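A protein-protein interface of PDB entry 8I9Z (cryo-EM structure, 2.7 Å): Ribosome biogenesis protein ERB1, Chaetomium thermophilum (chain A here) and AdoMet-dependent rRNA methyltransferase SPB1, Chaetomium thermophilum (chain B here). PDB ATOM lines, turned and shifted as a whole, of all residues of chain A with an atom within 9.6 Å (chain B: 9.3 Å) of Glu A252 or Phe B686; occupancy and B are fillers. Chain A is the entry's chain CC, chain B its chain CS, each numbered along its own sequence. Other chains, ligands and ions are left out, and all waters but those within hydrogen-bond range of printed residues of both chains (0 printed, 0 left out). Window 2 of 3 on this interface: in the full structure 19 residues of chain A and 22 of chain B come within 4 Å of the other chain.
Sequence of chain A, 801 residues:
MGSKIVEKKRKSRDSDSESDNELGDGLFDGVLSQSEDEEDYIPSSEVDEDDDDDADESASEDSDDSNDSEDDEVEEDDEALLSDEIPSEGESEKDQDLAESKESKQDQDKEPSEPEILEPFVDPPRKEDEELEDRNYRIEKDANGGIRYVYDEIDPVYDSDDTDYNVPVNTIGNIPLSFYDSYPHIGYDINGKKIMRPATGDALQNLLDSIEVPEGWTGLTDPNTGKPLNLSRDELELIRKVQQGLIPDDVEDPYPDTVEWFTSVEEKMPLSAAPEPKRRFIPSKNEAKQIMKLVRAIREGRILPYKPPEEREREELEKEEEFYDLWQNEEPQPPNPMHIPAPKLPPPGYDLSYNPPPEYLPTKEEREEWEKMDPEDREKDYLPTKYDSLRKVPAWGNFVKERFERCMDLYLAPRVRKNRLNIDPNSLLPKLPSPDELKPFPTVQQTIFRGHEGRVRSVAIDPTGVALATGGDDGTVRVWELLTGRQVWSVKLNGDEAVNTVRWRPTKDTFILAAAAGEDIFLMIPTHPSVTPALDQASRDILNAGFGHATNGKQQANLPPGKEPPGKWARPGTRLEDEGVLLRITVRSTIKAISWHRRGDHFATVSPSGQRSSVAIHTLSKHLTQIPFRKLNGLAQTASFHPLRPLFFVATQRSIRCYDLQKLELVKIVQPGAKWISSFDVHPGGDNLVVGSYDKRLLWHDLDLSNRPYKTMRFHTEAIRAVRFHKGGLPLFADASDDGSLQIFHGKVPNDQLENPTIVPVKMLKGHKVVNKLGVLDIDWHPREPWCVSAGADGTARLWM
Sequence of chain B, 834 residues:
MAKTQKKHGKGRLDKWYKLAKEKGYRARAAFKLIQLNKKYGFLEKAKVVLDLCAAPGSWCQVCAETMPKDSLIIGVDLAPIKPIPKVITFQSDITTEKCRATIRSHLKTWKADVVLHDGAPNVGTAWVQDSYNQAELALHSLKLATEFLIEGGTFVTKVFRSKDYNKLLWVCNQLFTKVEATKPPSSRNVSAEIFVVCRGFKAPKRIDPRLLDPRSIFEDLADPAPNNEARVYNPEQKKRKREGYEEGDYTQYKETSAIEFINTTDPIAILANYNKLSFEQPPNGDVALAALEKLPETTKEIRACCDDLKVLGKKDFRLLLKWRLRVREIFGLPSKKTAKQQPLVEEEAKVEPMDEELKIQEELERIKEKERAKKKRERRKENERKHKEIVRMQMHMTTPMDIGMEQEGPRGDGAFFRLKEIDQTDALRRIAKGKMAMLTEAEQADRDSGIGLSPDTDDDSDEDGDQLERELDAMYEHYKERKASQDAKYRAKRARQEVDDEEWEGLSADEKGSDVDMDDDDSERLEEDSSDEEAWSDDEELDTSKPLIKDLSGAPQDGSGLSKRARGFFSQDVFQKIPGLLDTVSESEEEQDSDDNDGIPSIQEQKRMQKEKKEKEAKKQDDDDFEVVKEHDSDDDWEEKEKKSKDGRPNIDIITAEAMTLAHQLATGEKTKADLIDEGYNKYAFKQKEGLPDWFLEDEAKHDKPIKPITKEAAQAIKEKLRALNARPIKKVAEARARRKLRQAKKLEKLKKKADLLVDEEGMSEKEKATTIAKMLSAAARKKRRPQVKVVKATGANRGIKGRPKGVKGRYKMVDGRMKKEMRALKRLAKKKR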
ATOM      1  N   LYS A 241      10.330 -23.417  -7.816  1.00  0.00           N
ATOM      2  CA  LYS A 241      10.706 -23.949  -6.512  1.00  0.00           C
ATOM      3  C   LYS A 241      12.103 -24.561  -6.536  1.00  0.00           C
ATOM      4  O   LYS A 241      12.864 -24.419  -5.573  1.00  0.00           O
ATOM      5  CB  LYS A 241       9.661 -24.971  -6.071  1.00  0.00           C
ATOM      6  CG  LYS A 241       8.613 -24.405  -5.127  1.00  0.00           C
ATOM      7  CD  LYS A 241       7.533 -25.423  -4.761  1.00  0.00           C
ATOM      8  CE  LYS A 241       7.993 -26.440  -3.722  1.00  0.00           C
ATOM      9  NZ  LYS A 241       8.759 -27.583  -4.297  1.00  0.00           N
ATOM     10  N   GLN A 244      14.961 -21.388  -7.276  1.00  0.00           N
ATOM     11  CA  GLN A 244      15.281 -20.560  -6.117  1.00  0.00           C
ATOM     12  C   GLN A 244      15.647 -21.412  -4.908  1.00  0.00           C
ATOM     13  O   GLN A 244      16.532 -21.043  -4.129  1.00  0.00           O
ATOM     14  CB  GLN A 244      14.121 -19.625  -5.784  1.00  0.00           C
ATOM     15  CG  GLN A 244      13.383 -19.097  -6.993  1.00  0.00           C
ATOM     16  CD  GLN A 244      12.910 -17.672  -6.815  1.00  0.00           C
ATOM     17  OE1 GLN A 244      13.250 -16.792  -7.603  1.00  0.00           O
ATOM     18  NE2 GLN A 244      12.134 -17.432  -5.768  1.00  0.00           N
ATOM     19  N   GLY A 245      14.980 -22.548  -4.732  1.00  0.00           N
ATOM     20  CA  GLY A 245      15.290 -23.423  -3.622  1.00  0.00           C
ATOM     21  C   GLY A 245      14.876 -22.904  -2.269  1.00  0.00           C
ATOM     22  O   GLY A 245      15.444 -23.326  -1.258  1.00  0.00           O
ATOM     23  N   LEU A 246      13.904 -21.990  -2.215  1.00  0.00           N
ATOM     24  CA  LEU A 246      13.516 -21.385  -0.944  1.00  0.00           C
ATOM     25  C   LEU A 246      12.758 -22.371  -0.060  1.00  0.00           C
ATOM     26  O   LEU A 246      12.976 -22.418   1.155  1.00  0.00           O
ATOM     27  CB  LEU A 246      12.716 -20.096  -1.202  1.00  0.00           C
ATOM     28  CG  LEU A 246      11.449 -19.934  -2.066  1.00  0.00           C
ATOM     29  CD1 LEU A 246      10.169 -20.539  -1.495  1.00  0.00           C
ATOM     30  CD2 LEU A 246      11.231 -18.461  -2.388  1.00  0.00           C
ATOM     31  N   ILE A 247      11.877 -23.172  -0.653  1.00  0.00           N
ATOM     32  CA  ILE A 247      11.151 -24.228   0.052  1.00  0.00           C
ATOM     33  C   ILE A 247      11.125 -25.448  -0.861  1.00  0.00           C
ATOM     34  O   ILE A 247      10.523 -25.392  -1.943  1.00  0.00           O
ATOM     35  CB  ILE A 247       9.727 -23.793   0.443  1.00  0.00           C
ATOM     36  CG1 ILE A 247       9.747 -22.709   1.525  1.00  0.00           C
ATOM     37  CG2 ILE A 247       8.924 -24.982   0.936  1.00  0.00           C
ATOM     38  CD1 ILE A 247       8.377 -22.190   1.902  1.00  0.00           C
ATOM     39  N   PRO A 248      11.796 -26.544  -0.495  1.00  0.00           N
ATOM     40  CA  PRO A 248      11.772 -27.742  -1.352  1.00  0.00           C
ATOM     41  C   PRO A 248      10.394 -28.368  -1.518  1.00  0.00           C
ATOM     42  O   PRO A 248      10.082 -28.874  -2.603  1.00  0.00           O
ATOM     43  CB  PRO A 248      12.740 -28.693  -0.635  1.00  0.00           C
ATOM     44  CG  PRO A 248      13.627 -27.801   0.165  1.00  0.00           C
ATOM     45  CD  PRO A 248      12.748 -26.681   0.619  1.00  0.00           C
ATOM     46  N   ASP A 249       9.557 -28.343  -0.481  1.00  0.00           N
ATOM     47  CA  ASP A 249       8.243 -28.966  -0.552  1.00  0.00           C
ATOM     48  C   ASP A 249       7.311 -28.310   0.456  1.00  0.00           C
ATOM     49  O   ASP A 249       7.720 -27.959   1.566  1.00  0.00           O
ATOM     50  CB  ASP A 249       8.320 -30.476  -0.294  1.00  0.00           C
ATOM     51  CG  ASP A 249       7.208 -31.242  -0.979  1.00  0.00           C
ATOM     52  OD1 ASP A 249       6.501 -30.645  -1.819  1.00  0.00           O
ATOM     53  OD2 ASP A 249       7.039 -32.443  -0.680  1.00  0.00           O
ATOM     54  N   ASP A 250       6.047 -28.171   0.063  1.00  0.00           N
ATOM     55  CA  ASP A 250       5.047 -27.506   0.883  1.00  0.00           C
ATOM     56  C   ASP A 250       4.628 -28.399   2.049  1.00  0.00           C
ATOM     57  O   ASP A 250       4.965 -29.587   2.109  1.00  0.00           O
ATOM     58  CB  ASP A 250       3.844 -27.113   0.029  1.00  0.00           C
ATOM     59  CG  ASP A 250       4.236 -26.715  -1.381  1.00  0.00           C
ATOM     60  OD1 ASP A 250       4.893 -25.665  -1.542  1.00  0.00           O
ATOM     61  OD2 ASP A 250       3.888 -27.451  -2.327  1.00  0.00           O
ATOM     62  N   VAL A 251       3.858 -27.807   2.974  1.00  0.00           N
ATOM     63  CA  VAL A 251       3.408 -28.416   4.228  1.00  0.00           C
ATOM     64  C   VAL A 251       4.611 -28.943   5.000  1.00  0.00           C
ATOM     65  O   VAL A 251       4.891 -30.148   4.995  1.00  0.00           O
ATOM     66  CB  VAL A 251       2.359 -29.524   3.994  1.00  0.00           C
ATOM     67  CG1 VAL A 251       1.646 -29.864   5.296  1.00  0.00           C
ATOM     68  CG2 VAL A 251       1.344 -29.091   2.942  1.00  0.00           C
ATOM     69  N   GLU A 252       5.338 -28.044   5.657  1.00  0.00           N
ATOM     70  CA  GLU A 252       6.608 -28.395   6.278  1.00  0.00           C
ATOM     71  C   GLU A 252       6.890 -27.418   7.410  1.00  0.00           C
ATOM     72  O   GLU A 252       6.269 -26.356   7.516  1.00  0.00           O
ATOM     73  CB  GLU A 252       7.737 -28.384   5.243  1.00  0.00           C
ATOM     74  CG  GLU A 252       8.567 -29.654   5.205  1.00  0.00           C
ATOM     75  CD  GLU A 252       9.568 -29.656   4.067  1.00  0.00           C
ATOM     76  OE1 GLU A 252      10.141 -28.585   3.775  1.00  0.00           O
ATOM     77  OE2 GLU A 252       9.784 -30.729   3.464  1.00  0.00           O
ATOM     78  N   ASP A 253       7.837 -27.794   8.266  1.00  0.00           N
ATOM     79  CA  ASP A 253       8.391 -26.908   9.288  1.00  0.00           C
ATOM     80  C   ASP A 253       9.866 -26.721   8.967  1.00  0.00           C
ATOM     81  O   ASP A 253      10.664 -27.659   9.143  1.00  0.00           O
ATOM     82  CB  ASP A 253       8.205 -27.479  10.688  1.00  0.00           C
ATOM     83  CG  ASP A 253       8.416 -26.442  11.774  1.00  0.00           C
ATOM     84  OD1 ASP A 253       8.622 -25.257  11.437  1.00  0.00           O
ATOM     85  OD2 ASP A 253       8.378 -26.813  12.966  1.00  0.00           O
ATOM     86  N   PRO A 254      10.266 -25.543   8.477  1.00  0.00           N
ATOM     87  CA  PRO A 254      11.663 -25.359   8.055  1.00  0.00           C
ATOM     88  C   PRO A 254      12.658 -25.382   9.197  1.00  0.00           C
ATOM     89  O   PRO A 254      13.832 -25.691   8.962  1.00  0.00           O
ATOM     90  CB  PRO A 254      11.643 -23.992   7.365  1.00  0.00           C
ATOM     91  CG  PRO A 254      10.503 -23.277   7.995  1.00  0.00           C
ATOM     92  CD  PRO A 254       9.474 -24.313   8.328  1.00  0.00           C
ATOM     93  N   TYR A 255      12.235 -25.068  10.418  1.00  0.00           N
ATOM     94  CA  TYR A 255      13.092 -25.126  11.600  1.00  0.00           C
ATOM     95  C   TYR A 255      12.372 -25.929  12.671  1.00  0.00           C
ATOM     96  O   TYR A 255      11.781 -25.363  13.599  1.00  0.00           O
ATOM     97  CB  TYR A 255      13.448 -23.727  12.101  1.00  0.00           C
ATOM     98  CG  TYR A 255      13.711 -22.741  10.994  1.00  0.00           C
ATOM     99  CD1 TYR A 255      14.918 -22.733  10.319  1.00  0.00           C
ATOM    100  CD2 TYR A 255      12.747 -21.820  10.624  1.00  0.00           C
ATOM    101  CE1 TYR A 255      15.160 -21.830   9.307  1.00  0.00           C
ATOM    102  CE2 TYR A 255      12.976 -20.918   9.614  1.00  0.00           C
ATOM    103  CZ  TYR A 255      14.184 -20.927   8.961  1.00  0.00           C
ATOM    104  OH  TYR A 255      14.414 -20.027   7.953  1.00  0.00           O
ATOM    105  N   PRO A 256      12.401 -27.254  12.574  1.00  0.00           N
ATOM    106  CA  PRO A 256      11.722 -28.077  13.575  1.00  0.00           C
ATOM    107  C   PRO A 256      12.486 -28.101  14.886  1.00  0.00           C
ATOM    108  O   PRO A 256      13.703 -27.913  14.931  1.00  0.00           O
ATOM    109  CB  PRO A 256      11.688 -29.464  12.929  1.00  0.00           C
ATOM    110  CG  PRO A 256      12.801 -29.463  11.939  1.00  0.00           C
ATOM    111  CD  PRO A 256      13.224 -28.058  11.656  1.00  0.00           C
ATOM    112  N   ILE B 677      11.379 -33.118  -7.398  1.00  0.00           N
ATOM    113  CA  ILE B 677      11.137 -32.863  -5.982  1.00  0.00           C
ATOM    114  C   ILE B 677      12.229 -33.503  -5.138  1.00  0.00           C
ATOM    115  O   ILE B 677      12.737 -32.903  -4.183  1.00  0.00           O
ATOM    116  CB  ILE B 677       9.738 -33.373  -5.587  1.00  0.00           C
ATOM    117  CG1 ILE B 677       8.662 -32.529  -6.265  1.00  0.00           C
ATOM    118  CG2 ILE B 677       9.546 -33.337  -4.080  1.00  0.00           C
ATOM    119  CD1 ILE B 677       7.269 -33.059  -6.054  1.00  0.00           C
ATOM    120  N   ASP B 678      12.619 -34.728  -5.495  1.00  0.00           N
ATOM    121  CA  ASP B 678      13.605 -35.466  -4.715  1.00  0.00           C
ATOM    122  C   ASP B 678      14.983 -34.824  -4.797  1.00  0.00           C
ATOM    123  O   ASP B 678      15.704 -34.752  -3.796  1.00  0.00           O
ATOM    124  CB  ASP B 678      13.661 -36.916  -5.192  1.00  0.00           C
ATOM    125  CG  ASP B 678      12.981 -37.867  -4.235  1.00  0.00           C
ATOM    126  OD1 ASP B 678      12.369 -37.392  -3.256  1.00  0.00           O
ATOM    127  OD2 ASP B 678      13.058 -39.092  -4.460  1.00  0.00           O
ATOM    128  N   GLY B 680      15.607 -31.707  -5.292  1.00  0.00           N
ATOM    129  CA  GLY B 680      15.613 -30.399  -4.670  1.00  0.00           C
ATOM    130  C   GLY B 680      16.026 -30.392  -3.217  1.00  0.00           C
ATOM    131  O   GLY B 680      16.169 -29.317  -2.632  1.00  0.00           O
ATOM    132  N   TYR B 681      16.207 -31.567  -2.622  1.00  0.00           N
ATOM    133  CA  TYR B 681      16.729 -31.684  -1.265  1.00  0.00           C
ATOM    134  C   TYR B 681      18.246 -31.825  -1.349  1.00  0.00           C
ATOM    135  O   TYR B 681      18.812 -32.914  -1.254  1.00  0.00           O
ATOM    136  CB  TYR B 681      16.090 -32.864  -0.547  1.00  0.00           C
ATOM    137  CG  TYR B 681      14.678 -32.613  -0.071  1.00  0.00           C
ATOM    138  CD1 TYR B 681      13.599 -32.731  -0.935  1.00  0.00           C
ATOM    139  CD2 TYR B 681      14.422 -32.270   1.247  1.00  0.00           C
ATOM    140  CE1 TYR B 681      12.313 -32.507  -0.500  1.00  0.00           C
ATOM    141  CE2 TYR B 681      13.140 -32.046   1.688  1.00  0.00           C
ATOM    142  CZ  TYR B 681      12.093 -32.160   0.810  1.00  0.00           C
ATOM    143  OH  TYR B 681      10.817 -31.936   1.256  1.00  0.00           O
ATOM    144  N   ASN B 682      18.913 -30.690  -1.543  1.00  0.00           N
ATOM    145  CA  ASN B 682      20.361 -30.675  -1.685  1.00  0.00           C
ATOM    146  C   ASN B 682      20.990 -29.696  -0.705  1.00  0.00           C
ATOM    147  O   ASN B 682      20.322 -29.212   0.210  1.00  0.00           O
ATOM    148  CB  ASN B 682      20.773 -30.320  -3.111  1.00  0.00           C
ATOM    149  CG  ASN B 682      20.061 -29.095  -3.639  1.00  0.00           C
ATOM    150  OD1 ASN B 682      20.598 -27.991  -3.599  1.00  0.00           O
ATOM    151  ND2 ASN B 682      18.866 -29.286  -4.178  1.00  0.00           N
ATOM    152  N   LYS B 683      22.282 -29.415  -0.879  1.00  0.00           N
ATOM    153  CA  LYS B 683      22.993 -28.540   0.045  1.00  0.00           C
ATOM    154  C   LYS B 683      22.553 -27.089  -0.061  1.00  0.00           C
ATOM    155  O   LYS B 683      22.753 -26.327   0.889  1.00  0.00           O
ATOM    156  CB  LYS B 683      24.497 -28.638  -0.196  1.00  0.00           C
ATOM    157  CG  LYS B 683      24.905 -28.348  -1.621  1.00  0.00           C
ATOM    158  CD  LYS B 683      26.299 -28.856  -1.911  1.00  0.00           C
ATOM    159  CE  LYS B 683      27.025 -27.938  -2.872  1.00  0.00           C
ATOM    160  NZ  LYS B 683      28.474 -27.834  -2.546  1.00  0.00           N
ATOM    161  N   TYR B 684      21.954 -26.688  -1.182  1.00  0.00           N
ATOM    162  CA  TYR B 684      21.434 -25.339  -1.356  1.00  0.00           C
ATOM    163  C   TYR B 684      20.002 -25.214  -0.861  1.00  0.00           C
ATOM    164  O   TYR B 684      19.357 -24.183  -1.071  1.00  0.00           O
ATOM    165  CB  TYR B 684      21.525 -24.910  -2.820  1.00  0.00           C
ATOM    166  CG  TYR B 684      22.913 -24.974  -3.401  1.00  0.00           C
ATOM    167  CD1 TYR B 684      23.888 -24.073  -3.011  1.00  0.00           C
ATOM    168  CD2 TYR B 684      23.244 -25.928  -4.349  1.00  0.00           C
ATOM    169  CE1 TYR B 684      25.153 -24.125  -3.539  1.00  0.00           C
ATOM    170  CE2 TYR B 684      24.507 -25.988  -4.885  1.00  0.00           C
ATOM    171  CZ  TYR B 684      25.458 -25.084  -4.476  1.00  0.00           C
ATOM    172  OH  TYR B 684      26.726 -25.138  -5.008  1.00  0.00           O
ATOM    173  N   ALA B 685      19.491 -26.246  -0.208  1.00  0.00           N
ATOM    174  CA  ALA B 685      18.131 -26.259   0.295  1.00  0.00           C
ATOM    175  C   ALA B 685      18.140 -25.970   1.786  1.00  0.00           C
ATOM    176  O   ALA B 685      19.158 -26.150   2.458  1.00  0.00           O
ATOM    177  CB  ALA B 685      17.444 -27.602   0.028  1.00  0.00           C
ATOM    178  N   PHE B 686      16.989 -25.507   2.278  1.00  0.00           N
ATOM    179  CA  PHE B 686      16.771 -25.137   3.674  1.00  0.00           C
ATOM    180  C   PHE B 686      17.709 -24.023   4.132  1.00  0.00           C
ATOM    181  O   PHE B 686      18.114 -23.983   5.294  1.00  0.00           O
ATOM    182  CB  PHE B 686      16.884 -26.352   4.598  1.00  0.00           C
ATOM    183  CG  PHE B 686      15.840 -27.393   4.350  1.00  0.00           C
ATOM    184  CD1 PHE B 686      14.498 -27.088   4.467  1.00  0.00           C
ATOM    185  CD2 PHE B 686      16.200 -28.674   3.982  1.00  0.00           C
ATOM    186  CE1 PHE B 686      13.535 -28.047   4.233  1.00  0.00           C
ATOM    187  CE2 PHE B 686      15.247 -29.634   3.746  1.00  0.00           C
ATOM    188  CZ  PHE B 686      13.913 -29.322   3.872  1.00  0.00           C
ATOM    189  N   LYS B 687      18.059 -23.112   3.227  1.00  0.00           N
ATOM    190  CA  LYS B 687      18.854 -21.932   3.540  1.00  0.00           C
ATOM    191  C   LYS B 687      17.930 -20.722   3.523  1.00  0.00           C
ATOM    192  O   LYS B 687      17.283 -20.450   2.507  1.00  0.00           O
ATOM    193  CB  LYS B 687      19.992 -21.748   2.538  1.00  0.00           C
ATOM    194  CG  LYS B 687      21.184 -22.650   2.771  1.00  0.00           C
ATOM    195  CD  LYS B 687      22.241 -22.529   1.675  1.00  0.00           C
ATOM    196  CE  LYS B 687      22.378 -21.111   1.146  1.00  0.00           C
ATOM    197  NZ  LYS B 687      23.719 -20.875   0.545  1.00  0.00           N
ATOM    198  N   GLN B 688      17.874 -20.001   4.635  1.00  0.00           N
ATOM    199  CA  GLN B 688      16.954 -18.882   4.740  1.00  0.00           C
ATOM    200  C   GLN B 688      17.502 -17.662   4.016  1.00  0.00           C
ATOM    201  O   GLN B 688      18.713 -17.471   3.897  1.00  0.00           O
ATOM    202  CB  GLN B 688      16.704 -18.533   6.196  1.00  0.00           C
ATOM    203  CG  GLN B 688      17.964 -18.355   6.954  1.00  0.00           C
ATOM    204  CD  GLN B 688      17.859 -17.268   7.982  1.00  0.00           C
ATOM    205  OE1 GLN B 688      18.465 -17.327   9.045  1.00  0.00           O
ATOM    206  NE2 GLN B 688      17.060 -16.280   7.682  1.00  0.00           N
ATOM    207  N   LYS B 689      16.581 -16.848   3.489  1.00  0.00           N
ATOM    208  CA  LYS B 689      16.938 -15.592   2.845  1.00  0.00           C
ATOM    209  C   LYS B 689      16.004 -14.459   3.251  1.00  0.00           C
ATOM    210  O   LYS B 689      15.954 -13.442   2.549  1.00  0.00           O
ATOM    211  CB  LYS B 689      16.928 -15.714   1.305  1.00  0.00           C
ATOM    212  CG  LYS B 689      17.197 -17.098   0.741  1.00  0.00           C
ATOM    213  CD  LYS B 689      17.650 -17.050  -0.696  1.00  0.00           C
ATOM    214  CE  LYS B 689      18.258 -18.379  -1.091  1.00  0.00           C
ATOM    215  NZ  LYS B 689      19.216 -18.862  -0.061  1.00  0.00           N
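Hydrophobic or aromatic side chains of chain A within 4 Å of the printed part of chain B: Pro A248 and Tyr A255.
Among the printed residues, no Asp or Glu carboxylate lies within 4 Å of a Lys or Arg side-chain nitrogen of the other chain.
The backbone carbonyl oxygen (O) of Pro A248 lies within hydrogen-bond range of the side-chain amino group (NZ) of Lys A241, at 2.5 Å.
Among the printed residues, merely in contact across the chains: Tyr A255 with Gln B688 (3.3 Å), Asp A249 with Tyr B681 (3.3 Å), Glu A252 with Phe B686 (3.5 Å), Pro A248 with Tyr B681 (3.8 Å), Pro A248 with Ala B685 (3.8 Å) and Pro A248 with Phe B686 (3.9 Å).
Of the printed residues of chain B, Pro A248 touches Tyr B681 (3.8 Å), Ala B685 (3.8 Å) and Phe B686 (3.9 Å).
Of the printed residues of chain B, Asp A249 touches Tyr B681 (3.3 Å).
No residue of chain B comes within 4 Å of Val A251.
Of the printed residues of chain B, Glu A252 touches Tyr B681 and Phe B686.
Asp A253 touches none of the printed residues of chain B.
Printed residues of chain B within 4 Å of Tyr A255: Gln B688 (3.3 Å).
Phe B686 touches just these residues of chain A: Pro A248 (3.9 Å) and Glu A252 (3.5 Å).
Printed residues of chain A within 4 Å of Gln B688: Tyr A255.
The nearest residue of chain B that does not touch Glu A252 is Ile B677 (8.0 Å).
The nearest residue of chain A that does not touch Phe B686 is Gly A245 (4.4 Å).
OH of Tyr B681 lies within hydrogen-bond range of OE2 of Glu A252 (2.7 Å).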
